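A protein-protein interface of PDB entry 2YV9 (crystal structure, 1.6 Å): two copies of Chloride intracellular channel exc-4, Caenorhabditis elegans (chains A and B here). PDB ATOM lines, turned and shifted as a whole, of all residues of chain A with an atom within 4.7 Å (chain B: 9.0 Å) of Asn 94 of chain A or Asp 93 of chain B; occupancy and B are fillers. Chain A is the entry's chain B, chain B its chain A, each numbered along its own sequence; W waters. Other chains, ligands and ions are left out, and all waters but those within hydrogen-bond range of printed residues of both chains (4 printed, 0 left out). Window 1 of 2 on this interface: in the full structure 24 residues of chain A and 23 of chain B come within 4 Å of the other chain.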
ATOM      1  N   PHE A  39      11.927 -24.641  21.183  1.00  0.00           N
ATOM      2  CA  PHE A  39      12.084 -23.317  20.528  1.00  0.00           C
ATOM      3  C   PHE A  39      13.543 -23.075  20.128  1.00  0.00           C
ATOM      4  O   PHE A  39      13.825 -22.504  19.076  1.00  0.00           O
ATOM      5  CB  PHE A  39      11.540 -22.218  21.426  1.00  0.00           C
ATOM      6  CG  PHE A  39      10.119 -22.462  21.842  1.00  0.00           C
ATOM      7  CD1 PHE A  39       9.102 -22.165  20.967  1.00  0.00           C
ATOM      8  CD2 PHE A  39       9.799 -23.009  23.050  1.00  0.00           C
ATOM      9  CE1 PHE A  39       7.756 -22.403  21.325  1.00  0.00           C
ATOM     10  CE2 PHE A  39       8.462 -23.252  23.402  1.00  0.00           C
ATOM     11  CZ  PHE A  39       7.469 -22.938  22.550  1.00  0.00           C
ATOM     12  N   PHE A  43      14.576 -22.524  16.031  1.00  0.00           N
ATOM     13  CA  PHE A  43      15.469 -21.506  15.474  1.00  0.00           C
ATOM     14  C   PHE A  43      16.806 -22.040  14.968  1.00  0.00           C
ATOM     15  O   PHE A  43      17.349 -21.516  13.978  1.00  0.00           O
ATOM     16  CB  PHE A  43      15.652 -20.333  16.383  1.00  0.00           C
ATOM     17  CG  PHE A  43      14.369 -19.633  16.686  1.00  0.00           C
ATOM     18  CD1 PHE A  43      13.560 -19.176  15.652  1.00  0.00           C
ATOM     19  CD2 PHE A  43      13.899 -19.545  17.997  1.00  0.00           C
ATOM     20  CE1 PHE A  43      12.349 -18.567  15.919  1.00  0.00           C
ATOM     21  CE2 PHE A  43      12.712 -18.875  18.267  1.00  0.00           C
ATOM     22  CZ  PHE A  43      11.917 -18.426  17.232  1.00  0.00           C
ATOM     23  N   PRO A  80      15.634 -19.712  23.762  1.00  0.00           N
ATOM     24  CA  PRO A  80      16.619 -19.209  22.807  1.00  0.00           C
ATOM     25  C   PRO A  80      16.861 -17.709  22.890  1.00  0.00           C
ATOM     26  O   PRO A  80      15.929 -16.953  23.137  1.00  0.00           O
ATOM     27  CB  PRO A  80      16.043 -19.591  21.454  1.00  0.00           C
ATOM     28  CG  PRO A  80      14.614 -19.726  21.689  1.00  0.00           C
ATOM     29  CD  PRO A  80      14.367 -20.078  23.087  1.00  0.00           C
ATOM     30  N   THR A  92      16.266 -11.403  22.442  1.00  0.00           N
ATOM     31  CA  THR A  92      15.891 -12.321  23.509  1.00  0.00           C
ATOM     32  C   THR A  92      14.463 -12.873  23.362  1.00  0.00           C
ATOM     33  O   THR A  92      14.115 -13.894  23.956  1.00  0.00           O
ATOM     34  CB  THR A  92      16.032 -11.720  24.913  1.00  0.00           C
ATOM     35  OG1 THR A  92      15.017 -10.728  25.132  1.00  0.00           O
ATOM     36  CG2 THR A  92      17.441 -11.170  25.116  1.00  0.00           C
ATOM     37  N   ASP A  93      13.637 -12.212  22.559  1.00  0.00           N
ATOM     38  CA  ASP A  93      12.241 -12.580  22.460  1.00  0.00           C
ATOM     39  C   ASP A  93      12.058 -13.350  21.161  1.00  0.00           C
ATOM     40  O   ASP A  93      12.667 -13.013  20.123  1.00  0.00           O
ATOM     41  CB  ASP A  93      11.387 -11.314  22.461  1.00  0.00           C
ATOM     42  CG  ASP A  93       9.887 -11.592  22.403  1.00  0.00           C
ATOM     43  OD1 ASP A  93       9.205 -11.383  23.435  1.00  0.00           O
ATOM     44  OD2 ASP A  93       9.401 -12.014  21.322  1.00  0.00           O
ATOM     45  N   ASN A  94      11.257 -14.396  21.219  1.00  0.00           N
ATOM     46  CA  ASN A  94      11.033 -15.244  20.045  1.00  0.00           C
ATOM     47  C   ASN A  94      10.500 -14.505  18.850  1.00  0.00           C
ATOM     48  O   ASN A  94      10.746 -14.877  17.703  1.00  0.00           O
ATOM     49  CB  ASN A  94      10.211 -16.496  20.392  1.00  0.00           C
ATOM     50  CG  ASN A  94      10.984 -17.465  21.294  1.00  0.00           C
ATOM     51  OD1 ASN A  94      12.122 -17.192  21.655  1.00  0.00           O
ATOM     52  ND2 ASN A  94      10.373 -18.575  21.641  1.00  0.00           N
ATOM     53  N   ARG A  95       9.758 -13.433  19.110  1.00  0.00           N
ATOM     54  CA  ARG A  95       9.259 -12.614  18.022  1.00  0.00           C
ATOM     55  C   ARG A  95      10.436 -11.942  17.309  1.00  0.00           C
ATOM     56  O   ARG A  95      10.432 -11.835  16.085  1.00  0.00           O
ATOM     57  CB  ARG A  95       8.269 -11.537  18.528  1.00  0.00           C
ATOM     58  CG  ARG A  95       6.964 -12.092  18.983  1.00  0.00           C
ATOM     59  CD  ARG A  95       6.153 -11.053  19.744  1.00  0.00           C
ATOM     60  NE  ARG A  95       6.788 -10.680  21.002  1.00  0.00           N
ATOM     61  CZ  ARG A  95       6.454  -9.623  21.733  1.00  0.00           C
ATOM     62  NH1 ARG A  95       5.436  -8.823  21.360  1.00  0.00           N
ATOM     63  NH2 ARG A  95       7.110  -9.353  22.848  1.00  0.00           N
ATOM     64  N   GLU A  96      11.397 -11.452  18.095  1.00  0.00           N
ATOM     65  CA  GLU A  96      12.604 -10.759  17.585  1.00  0.00           C
ATOM     66  C   GLU A  96      13.495 -11.719  16.823  1.00  0.00           C
ATOM     67  O   GLU A  96      13.982 -11.380  15.743  1.00  0.00           O
ATOM     68  CB  GLU A  96      13.413 -10.149  18.737  1.00  0.00           C
ATOM     69  CG  GLU A  96      12.746  -8.963  19.459  1.00  0.00           C
ATOM     70  CD  GLU A  96      13.330  -8.738  20.881  1.00  0.00           C
ATOM     71  OE1 GLU A  96      14.213  -9.507  21.357  1.00  0.00           O
ATOM     72  OE2 GLU A  96      12.874  -7.786  21.548  1.00  0.00           O
ATOM     73  N   ILE A  97      13.712 -12.918  17.377  1.00  0.00           N
ATOM     74  CA  ILE A  97      14.579 -13.916  16.720  1.00  0.00           C
ATOM     75  C   ILE A  97      13.972 -14.336  15.364  1.00  0.00           C
ATOM     76  O   ILE A  97      14.612 -14.270  14.310  1.00  0.00           O
ATOM     77  CB  ILE A  97      14.803 -15.141  17.636  1.00  0.00           C
ATOM     78  CG1 ILE A  97      15.419 -14.709  18.972  1.00  0.00           C
ATOM     79  CG2 ILE A  97      15.559 -16.226  16.915  1.00  0.00           C
ATOM     80  CD1 ILE A  97      15.562 -15.832  20.017  1.00  0.00           C
ATOM     81  N   GLU A  98      12.717 -14.710  15.373  1.00  0.00           N
ATOM     82  CA  GLU A  98      12.018 -15.067  14.150  1.00  0.00           C
ATOM     83  C   GLU A  98      12.024 -13.912  13.143  1.00  0.00           C
ATOM     84  O   GLU A  98      12.244 -14.128  11.943  1.00  0.00           O
ATOM     85  CB  GLU A  98      10.582 -15.442  14.459  1.00  0.00           C
ATOM     86  CG  GLU A  98       9.824 -15.865  13.237  1.00  0.00           C
ATOM     87  CD  GLU A  98       8.448 -16.297  13.589  1.00  0.00           C
ATOM     88  OE1 GLU A  98       8.203 -17.528  13.724  1.00  0.00           O
ATOM     89  OE2 GLU A  98       7.603 -15.390  13.779  1.00  0.00           O
ATOM     90  N   PHE B  39       7.575  -8.287  29.263  1.00  0.00           N
ATOM     91  CA  PHE B  39       6.687  -8.971  28.278  1.00  0.00           C
ATOM     92  C   PHE B  39       5.309  -9.204  28.891  1.00  0.00           C
ATOM     93  O   PHE B  39       4.307  -9.085  28.226  1.00  0.00           O
ATOM     94  CB  PHE B  39       7.372 -10.214  27.772  1.00  0.00           C
ATOM     95  CG  PHE B  39       8.689  -9.904  27.199  1.00  0.00           C
ATOM     96  CD1 PHE B  39       8.773  -9.206  26.004  1.00  0.00           C
ATOM     97  CD2 PHE B  39       9.839 -10.112  27.911  1.00  0.00           C
ATOM     98  CE1 PHE B  39      10.028  -8.856  25.468  1.00  0.00           C
ATOM     99  CE2 PHE B  39      11.070  -9.727  27.376  1.00  0.00           C
ATOM    100  CZ  PHE B  39      11.150  -9.121  26.158  1.00  0.00           C
ATOM    101  N   PHE B  43       1.749  -7.510  27.187  1.00  0.00           N
ATOM    102  CA  PHE B  43       0.518  -8.191  26.829  1.00  0.00           C
ATOM    103  C   PHE B  43      -0.643  -7.822  27.729  1.00  0.00           C
ATOM    104  O   PHE B  43      -1.809  -7.770  27.272  1.00  0.00           O
ATOM    105  CB  PHE B  43       0.676  -9.700  26.718  1.00  0.00           C
ATOM    106  CG  PHE B  43       1.632 -10.090  25.661  1.00  0.00           C
ATOM    107  CD1 PHE B  43       1.471  -9.622  24.371  1.00  0.00           C
ATOM    108  CD2 PHE B  43       2.721 -10.879  25.930  1.00  0.00           C
ATOM    109  CE1 PHE B  43       2.374  -9.951  23.389  1.00  0.00           C
ATOM    110  CE2 PHE B  43       3.610 -11.216  24.926  1.00  0.00           C
ATOM    111  CZ  PHE B  43       3.455 -10.753  23.684  1.00  0.00           C
ATOM    112  N   ALA B  77       7.600 -23.727  30.425  1.00  0.00           N
ATOM    113  CA  ALA B  77       7.310 -22.452  29.793  1.00  0.00           C
ATOM    114  C   ALA B  77       7.279 -21.373  30.851  1.00  0.00           C
ATOM    115  O   ALA B  77       6.891 -21.641  31.993  1.00  0.00           O
ATOM    116  CB  ALA B  77       5.988 -22.541  29.059  1.00  0.00           C
ATOM    117  N   GLN B  78       7.637 -20.132  30.468  1.00  0.00           N
ATOM    118  CA  GLN B  78       7.669 -19.027  31.415  1.00  0.00           C
ATOM    119  C   GLN B  78       6.591 -18.010  31.098  1.00  0.00           C
ATOM    120  O   GLN B  78       6.199 -17.878  29.891  1.00  0.00           O
ATOM    121  CB  GLN B  78       9.019 -18.281  31.302  1.00  0.00           C
ATOM    122  CG  GLN B  78      10.215 -19.152  31.692  1.00  0.00           C
ATOM    123  CD  GLN B  78      10.085 -19.672  33.103  1.00  0.00           C
ATOM    124  OE1 GLN B  78       9.983 -20.895  33.347  1.00  0.00           O
ATOM    125  NE2 GLN B  78      10.057 -18.761  34.054  1.00  0.00           N
ATOM    126  N   PRO B  79       6.155 -17.257  32.132  1.00  0.00           N
ATOM    127  CA  PRO B  79       5.261 -16.170  31.838  1.00  0.00           C
ATOM    128  C   PRO B  79       5.958 -15.191  30.936  1.00  0.00           C
ATOM    129  O   PRO B  79       7.181 -15.108  30.945  1.00  0.00           O
ATOM    130  CB  PRO B  79       4.963 -15.544  33.200  1.00  0.00           C
ATOM    131  CG  PRO B  79       5.320 -16.568  34.191  1.00  0.00           C
ATOM    132  CD  PRO B  79       6.424 -17.334  33.576  1.00  0.00           C
ATOM    133  N   PRO B  80       5.174 -14.460  30.122  1.00  0.00           N
ATOM    134  CA  PRO B  80       3.721 -14.533  30.016  1.00  0.00           C
ATOM    135  C   PRO B  80       3.217 -15.778  29.293  1.00  0.00           C
ATOM    136  O   PRO B  80       3.823 -16.272  28.321  1.00  0.00           O
ATOM    137  CB  PRO B  80       3.379 -13.323  29.154  1.00  0.00           C
ATOM    138  CG  PRO B  80       4.610 -13.120  28.319  1.00  0.00           C
ATOM    139  CD  PRO B  80       5.754 -13.508  29.146  1.00  0.00           C
ATOM    140  N   ILE B  81       2.090 -16.284  29.798  1.00  0.00           N
ATOM    141  CA  ILE B  81       1.382 -17.405  29.212  1.00  0.00           C
ATOM    142  C   ILE B  81      -0.111 -16.992  29.212  1.00  0.00           C
ATOM    143  O   ILE B  81      -0.611 -16.473  30.204  1.00  0.00           O
ATOM    144  CB  ILE B  81       1.529 -18.727  30.049  1.00  0.00           C
ATOM    145  CG1 ILE B  81       2.942 -19.249  29.898  1.00  0.00           C
ATOM    146  CG2 ILE B  81       0.617 -19.788  29.538  1.00  0.00           C
ATOM    147  CD1 ILE B  81       3.286 -20.264  30.977  1.00  0.00           C
ATOM    148  N   MET B  82      -0.818 -17.259  28.117  1.00  0.00           N
ATOM    149  CA  MET B  82      -2.222 -16.904  27.974  1.00  0.00           C
ATOM    150  C   MET B  82      -3.037 -18.147  27.689  1.00  0.00           C
ATOM    151  O   MET B  82      -2.626 -18.990  26.821  1.00  0.00           O
ATOM    152  CB  MET B  82      -2.427 -15.840  26.896  1.00  0.00           C
ATOM    153  CG  MET B  82      -3.834 -15.235  26.920  1.00  0.00           C
ATOM    154  SD  MET B  82      -3.953 -13.821  25.802  1.00  0.00           S
ATOM    155  CE  MET B  82      -3.852 -14.525  24.186  1.00  0.00           C
ATOM    156  N   THR B  90      -3.828 -22.984  24.778  1.00  0.00           N
ATOM    157  CA  THR B  90      -2.824 -22.442  25.663  1.00  0.00           C
ATOM    158  C   THR B  90      -1.744 -21.797  24.799  1.00  0.00           C
ATOM    159  O   THR B  90      -1.148 -22.455  23.961  1.00  0.00           O
ATOM    160  CB  THR B  90      -2.194 -23.529  26.525  1.00  0.00           C
ATOM    161  OG1 THR B  90      -3.229 -24.118  27.324  1.00  0.00           O
ATOM    162  CG2 THR B  90      -1.130 -22.959  27.425  1.00  0.00           C
ATOM    163  N   TYR B  91      -1.537 -20.498  24.959  1.00  0.00           N
ATOM    164  CA  TYR B  91      -0.519 -19.774  24.200  1.00  0.00           C
ATOM    165  C   TYR B  91       0.676 -19.518  25.107  1.00  0.00           C
ATOM    166  O   TYR B  91       0.654 -18.602  25.950  1.00  0.00           O
ATOM    167  CB  TYR B  91      -1.085 -18.443  23.694  1.00  0.00           C
ATOM    168  CG  TYR B  91      -2.479 -18.521  23.076  1.00  0.00           C
ATOM    169  CD1 TYR B  91      -2.652 -18.921  21.765  1.00  0.00           C
ATOM    170  CD2 TYR B  91      -3.605 -18.195  23.813  1.00  0.00           C
ATOM    171  CE1 TYR B  91      -3.934 -18.966  21.167  1.00  0.00           C
ATOM    172  CE2 TYR B  91      -4.908 -18.218  23.228  1.00  0.00           C
ATOM    173  CZ  TYR B  91      -5.055 -18.620  21.902  1.00  0.00           C
ATOM    174  OH  TYR B  91      -6.324 -18.708  21.303  1.00  0.00           O
ATOM    175  N   THR B  92       1.731 -20.320  24.951  1.00  0.00           N
ATOM    176  CA  THR B  92       2.891 -20.206  25.831  1.00  0.00           C
ATOM    177  C   THR B  92       4.010 -19.373  25.205  1.00  0.00           C
ATOM    178  O   THR B  92       4.856 -18.869  25.927  1.00  0.00           O
ATOM    179  CB  THR B  92       3.444 -21.590  26.249  1.00  0.00           C
ATOM    180  OG1 THR B  92       3.893 -22.291  25.087  1.00  0.00           O
ATOM    181  CG2 THR B  92       2.345 -22.389  26.954  1.00  0.00           C
ATOM    182  N   ASP B  93       3.983 -19.176  23.883  1.00  0.00           N
ATOM    183  CA  ASP B  93       5.041 -18.531  23.137  1.00  0.00           C
ATOM    184  C   ASP B  93       4.577 -17.132  22.807  1.00  0.00           C
ATOM    185  O   ASP B  93       3.398 -16.938  22.444  1.00  0.00           O
ATOM    186  CB  ASP B  93       5.350 -19.284  21.844  1.00  0.00           C
ATOM    187  CG  ASP B  93       6.535 -18.706  21.078  1.00  0.00           C
ATOM    188  OD1 ASP B  93       6.398 -17.607  20.500  1.00  0.00           O
ATOM    189  OD2 ASP B  93       7.625 -19.348  21.032  1.00  0.00           O
ATOM    190  N   ASN B  94       5.465 -16.158  22.948  1.00  0.00           N
ATOM    191  CA  ASN B  94       5.059 -14.739  22.759  1.00  0.00           C
ATOM    192  C   ASN B  94       4.518 -14.481  21.361  1.00  0.00           C
ATOM    193  O   ASN B  94       3.644 -13.576  21.160  1.00  0.00           O
ATOM    194  CB  ASN B  94       6.202 -13.772  23.153  1.00  0.00           C
ATOM    195  CG  ASN B  94       6.441 -13.729  24.669  1.00  0.00           C
ATOM    196  OD1 ASN B  94       5.788 -14.455  25.425  1.00  0.00           O
ATOM    197  ND2 ASN B  94       7.306 -12.831  25.114  1.00  0.00           N
ATOM    198  N   ARG B  95       4.991 -15.235  20.368  1.00  0.00           N
ATOM    199  CA  ARG B  95       4.434 -15.092  18.999  1.00  0.00           C
ATOM    200  C   ARG B  95       2.923 -15.479  19.000  1.00  0.00           C
ATOM    201  O   ARG B  95       2.095 -14.822  18.358  1.00  0.00           O
ATOM    202  CB  ARG B  95       5.197 -15.988  17.988  1.00  0.00           C
ATOM    203  CG  ARG B  95       6.629 -15.535  17.775  1.00  0.00           C
ATOM    204  CD  ARG B  95       7.456 -16.584  17.027  1.00  0.00           C
ATOM    205  NE  ARG B  95       7.708 -17.771  17.858  1.00  0.00           N
ATOM    206  CZ  ARG B  95       8.127 -18.940  17.394  1.00  0.00           C
ATOM    207  NH1 ARG B  95       8.471 -19.102  16.122  1.00  0.00           N
ATOM    208  NH2 ARG B  95       8.327 -19.953  18.240  1.00  0.00           N
ATOM    209  N   GLU B  96       2.590 -16.563  19.685  1.00  0.00           N
ATOM    210  CA  GLU B  96       1.227 -17.078  19.802  1.00  0.00           C
ATOM    211  C   GLU B  96       0.313 -16.096  20.553  1.00  0.00           C
ATOM    212  O   GLU B  96      -0.807 -15.805  20.112  1.00  0.00           O
ATOM    213  CB  GLU B  96       1.240 -18.410  20.555  1.00  0.00           C
ATOM    214  CG  GLU B  96       1.964 -19.539  19.839  1.00  0.00           C
ATOM    215  CD  GLU B  96       2.159 -20.781  20.743  1.00  0.00           C
ATOM    216  OE1 GLU B  96       2.159 -20.681  21.990  1.00  0.00           O
ATOM    217  OE2 GLU B  96       2.307 -21.874  20.179  1.00  0.00           O
ATOM    218  N   ILE B  97       0.803 -15.544  21.661  1.00  0.00           N
ATOM    219  CA  ILE B  97      -0.004 -14.612  22.488  1.00  0.00           C
ATOM    220  C   ILE B  97      -0.268 -13.380  21.651  1.00  0.00           C
ATOM    221  O   ILE B  97      -1.419 -12.945  21.527  1.00  0.00           O
ATOM    222  CB  ILE B  97       0.710 -14.243  23.810  1.00  0.00           C
ATOM    223  CG1 ILE B  97       0.934 -15.503  24.671  1.00  0.00           C
ATOM    224  CG2 ILE B  97      -0.038 -13.178  24.604  1.00  0.00           C
ATOM    225  CD1 ILE B  97       1.920 -15.249  25.857  1.00  0.00           C
ATOM    226  N   GLU B  98       0.766 -12.813  21.053  1.00  0.00           N
ATOM    227  CA  GLU B  98       0.577 -11.598  20.233  1.00  0.00           C
ATOM    228  C   GLU B  98      -0.375 -11.878  19.077  1.00  0.00           C
ATOM    229  O   GLU B  98      -1.215 -11.042  18.741  1.00  0.00           O
ATOM    230  CB  GLU B  98       1.865 -11.112  19.634  1.00  0.00           C
ATOM    231  CG  GLU B  98       1.751  -9.765  18.964  1.00  0.00           C
ATOM    232  CD  GLU B  98       3.087  -9.339  18.396  1.00  0.00           C
ATOM    233  OE1 GLU B  98       3.755  -8.536  19.042  1.00  0.00           O
ATOM    234  OE2 GLU B  98       3.525  -9.867  17.358  1.00  0.00           O
ATOM    235  N   GLY B  99      -0.198 -13.050  18.449  1.00  0.00           N
ATOM    236  CA  GLY B  99      -1.026 -13.474  17.290  1.00  0.00           C
ATOM    237  C   GLY B  99      -2.508 -13.475  17.619  1.00  0.00           C
ATOM    238  O   GLY B  99      -3.368 -13.008  16.844  1.00  0.00           O
ATOM    239  N   ARG B 100      -2.833 -14.000  18.776  1.00  0.00           N
ATOM    240  CA  ARG B 100      -4.240 -14.096  19.184  1.00  0.00           C
ATOM    241  C   ARG B 100      -4.800 -12.687  19.481  1.00  0.00           C
ATOM    242  O   ARG B 100      -5.929 -12.348  19.098  1.00  0.00           O
ATOM    243  CB  ARG B 100      -4.420 -15.026  20.386  1.00  0.00           C
ATOM    244  CG  ARG B 100      -5.898 -15.155  20.853  1.00  0.00           C
ATOM    245  CD  ARG B 100      -6.839 -15.644  19.717  1.00  0.00           C
ATOM    246  NE  ARG B 100      -8.173 -15.821  20.287  1.00  0.00           N
ATOM    247  CZ  ARG B 100      -9.317 -15.482  19.686  1.00  0.00           C
ATOM    248  NH1 ARG B 100      -9.323 -14.951  18.473  1.00  0.00           N
ATOM    249  NH2 ARG B 100     -10.471 -15.656  20.338  1.00  0.00           N
ATOM    250  N   ILE B 101      -4.013 -11.851  20.149  1.00  0.00           N
ATOM    251  CA  ILE B 101      -4.467 -10.484  20.481  1.00  0.00           C
ATOM    252  C   ILE B 101      -4.584  -9.667  19.193  1.00  0.00           C
ATOM    253  O   ILE B 101      -5.536  -8.900  19.034  1.00  0.00           O
ATOM    254  CB  ILE B 101      -3.554  -9.815  21.536  1.00  0.00           C
ATOM    255  CG1 ILE B 101      -3.439 -10.683  22.799  1.00  0.00           C
ATOM    256  CG2 ILE B 101      -4.067  -8.386  21.867  1.00  0.00           C
ATOM    257  CD1 ILE B 101      -2.327 -10.178  23.750  1.00  0.00           C
HETATM  258  O   HOH W   1       2.901  -6.872  21.012  1.00  0.00           O
HETATM  259  O   HOH W   2       8.258 -19.808  23.779  1.00  0.00           O
HETATM  260  O   HOH W   3       9.779 -19.739  13.118  1.00  0.00           O
HETATM  261  O   HOH W   4      10.612 -12.684  25.511  1.00  0.00           O
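Printed residues of chain B that touch a printed residue of chain A: Phe 39, Phe 43, Asp 93, Asn 94, Arg 95 and Glu 98.
Hydrophobic or aromatic side chains of chain B that line the printed part of chain A: Phe 39 and Phe 43.
Among the printed residues, 13 pairs touch across the chains.
Among the printed residues, Asp or Glu carboxylates within 4 Å of a Lys or Arg side-chain nitrogen of the other chain: Arg 95 of chain A with Glu 98 of chain B (2.9 Å) and Glu 98 of chain A with Arg 95 of chain B (2.9 Å).
Phe 43 of chain A touches Arg 95 of chain B, and with the chains exchanged Arg 95 of chain A touches Phe 43 of chain B.
Asn 94 of chain A touches Arg 95 of chain B, and with the chains exchanged Arg 95 of chain A touches Asn 94 of chain B.
Arg 95 of chain B touches its own counterpart, Arg 95 of chain A.
Arg 95 of chain A touches Glu 98 of chain B, and with the chains exchanged Glu 98 of chain A touches Arg 95 of chain B.
Of the 13 pairs that touch across the chains among the printed residues, 13 have their exchanged pair printed and touching as well.
NH2 of Arg 95 of chain B is in salt-bridge range of OD2 of Asp 93 of chain B, 2.9 Å away.
The guanidinium group of Arg 95 of chain A lies within salt-bridge range of the side-chain carboxylate of Asp 93 of chain A, at 3.0 Å.
N of Asp 93 of chain A sits at hydrogen-bond distance from OE1 of Glu 96 of chain A (3.0 Å).
N of Asp 93 of chain B is in hydrogen-bond range of OE1 of Glu 96 of chain B (3.0 Å).
The side-chain amide nitrogen (ND2) of Asn 94 of chain A sits at hydrogen-bond distance from the side-chain carboxylate (OD2) of Asp 93 of chain B (2.9 Å).
OE1 of Glu 98 of chain A is in salt-bridge range of NH1 of Arg 95 of chain B (2.9 Å).
OD1 of Asp 93 of chain A sits at hydrogen-bond distance from ND2 of Asn 94 of chain B, 2.9 Å away.
NH1 of Arg 95 of chain A lies within salt-bridge range of OE1 of Glu 98 of chain B (2.9 Å).
Asp 93 of chain B touches just these residues of chain A: Phe 39 (3.1 Å) and Asn 94 (2.9 Å).
Of chain B, only Phe 39 (3.3 Å) and Asn 94 (2.9 Å) come within 4 Å of Asp 93 of chain A.
Of the printed residues of chain A, Arg 95 of chain B touches Phe 39, Phe 43, Asn 94, Arg 95 and Glu 98.
Of the printed residues of chain B, Phe 39 of chain A touches Asp 93 and Arg 95.
The nearest residue of chain B that does not touch Asn 94 of chain A is Asn 94 of chain B (5.4 Å).
The nearest printed residue of chain A that does not touch Asp 93 of chain B is Arg 95 of chain A (5.5 Å).
Among the printed residues, merely in contact across the chains: Phe 39 of chain A with Asp 93 of chain B (3.1 Å), Asp 93 of chain A with Phe 39 of chain B (3.3 Å), Arg 95 of chain A with Phe 39 of chain B (3.6 Å), Phe 39 of chain A with Arg 95 of chain B (3.6 Å), Arg 95 of chain A with Phe 43 of chain B (3.6 Å), Arg 95 of chain A with Arg 95 of chain B (3.7 Å), Phe 43 of chain A with Arg 95 of chain B (3.7 Å), Asn 94 of chain A with Arg 95 of chain B (3.8 Å) and Arg 95 of chain A with Asn 94 of chain B (3.8 Å).
Water W1 bridges the side-chain carboxylate (OE1) of Glu 98 of chain B (2.7 Å) and the guanidinium group (NH1) of Arg 95 of chain A (3.2 Å).
Water W3 bridges the side-chain carboxylate (OE1) of Glu 98 of chain A (2.8 Å) and the guanidinium group (NH1) of Arg 95 of chain B (3.3 Å).
Water W4 lies within hydrogen-bond range of OD1 of Asp 93 of chain A (2.8 Å) and ND2 of Asn 94 of chain B (3.3 Å).
Water W2 bridges the side-chain carboxylate (OD2) of Asp 93 of chain B (2.9 Å) and the side-chain amide nitrogen (ND2) of Asn 94 of chain A (3.3 Å).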
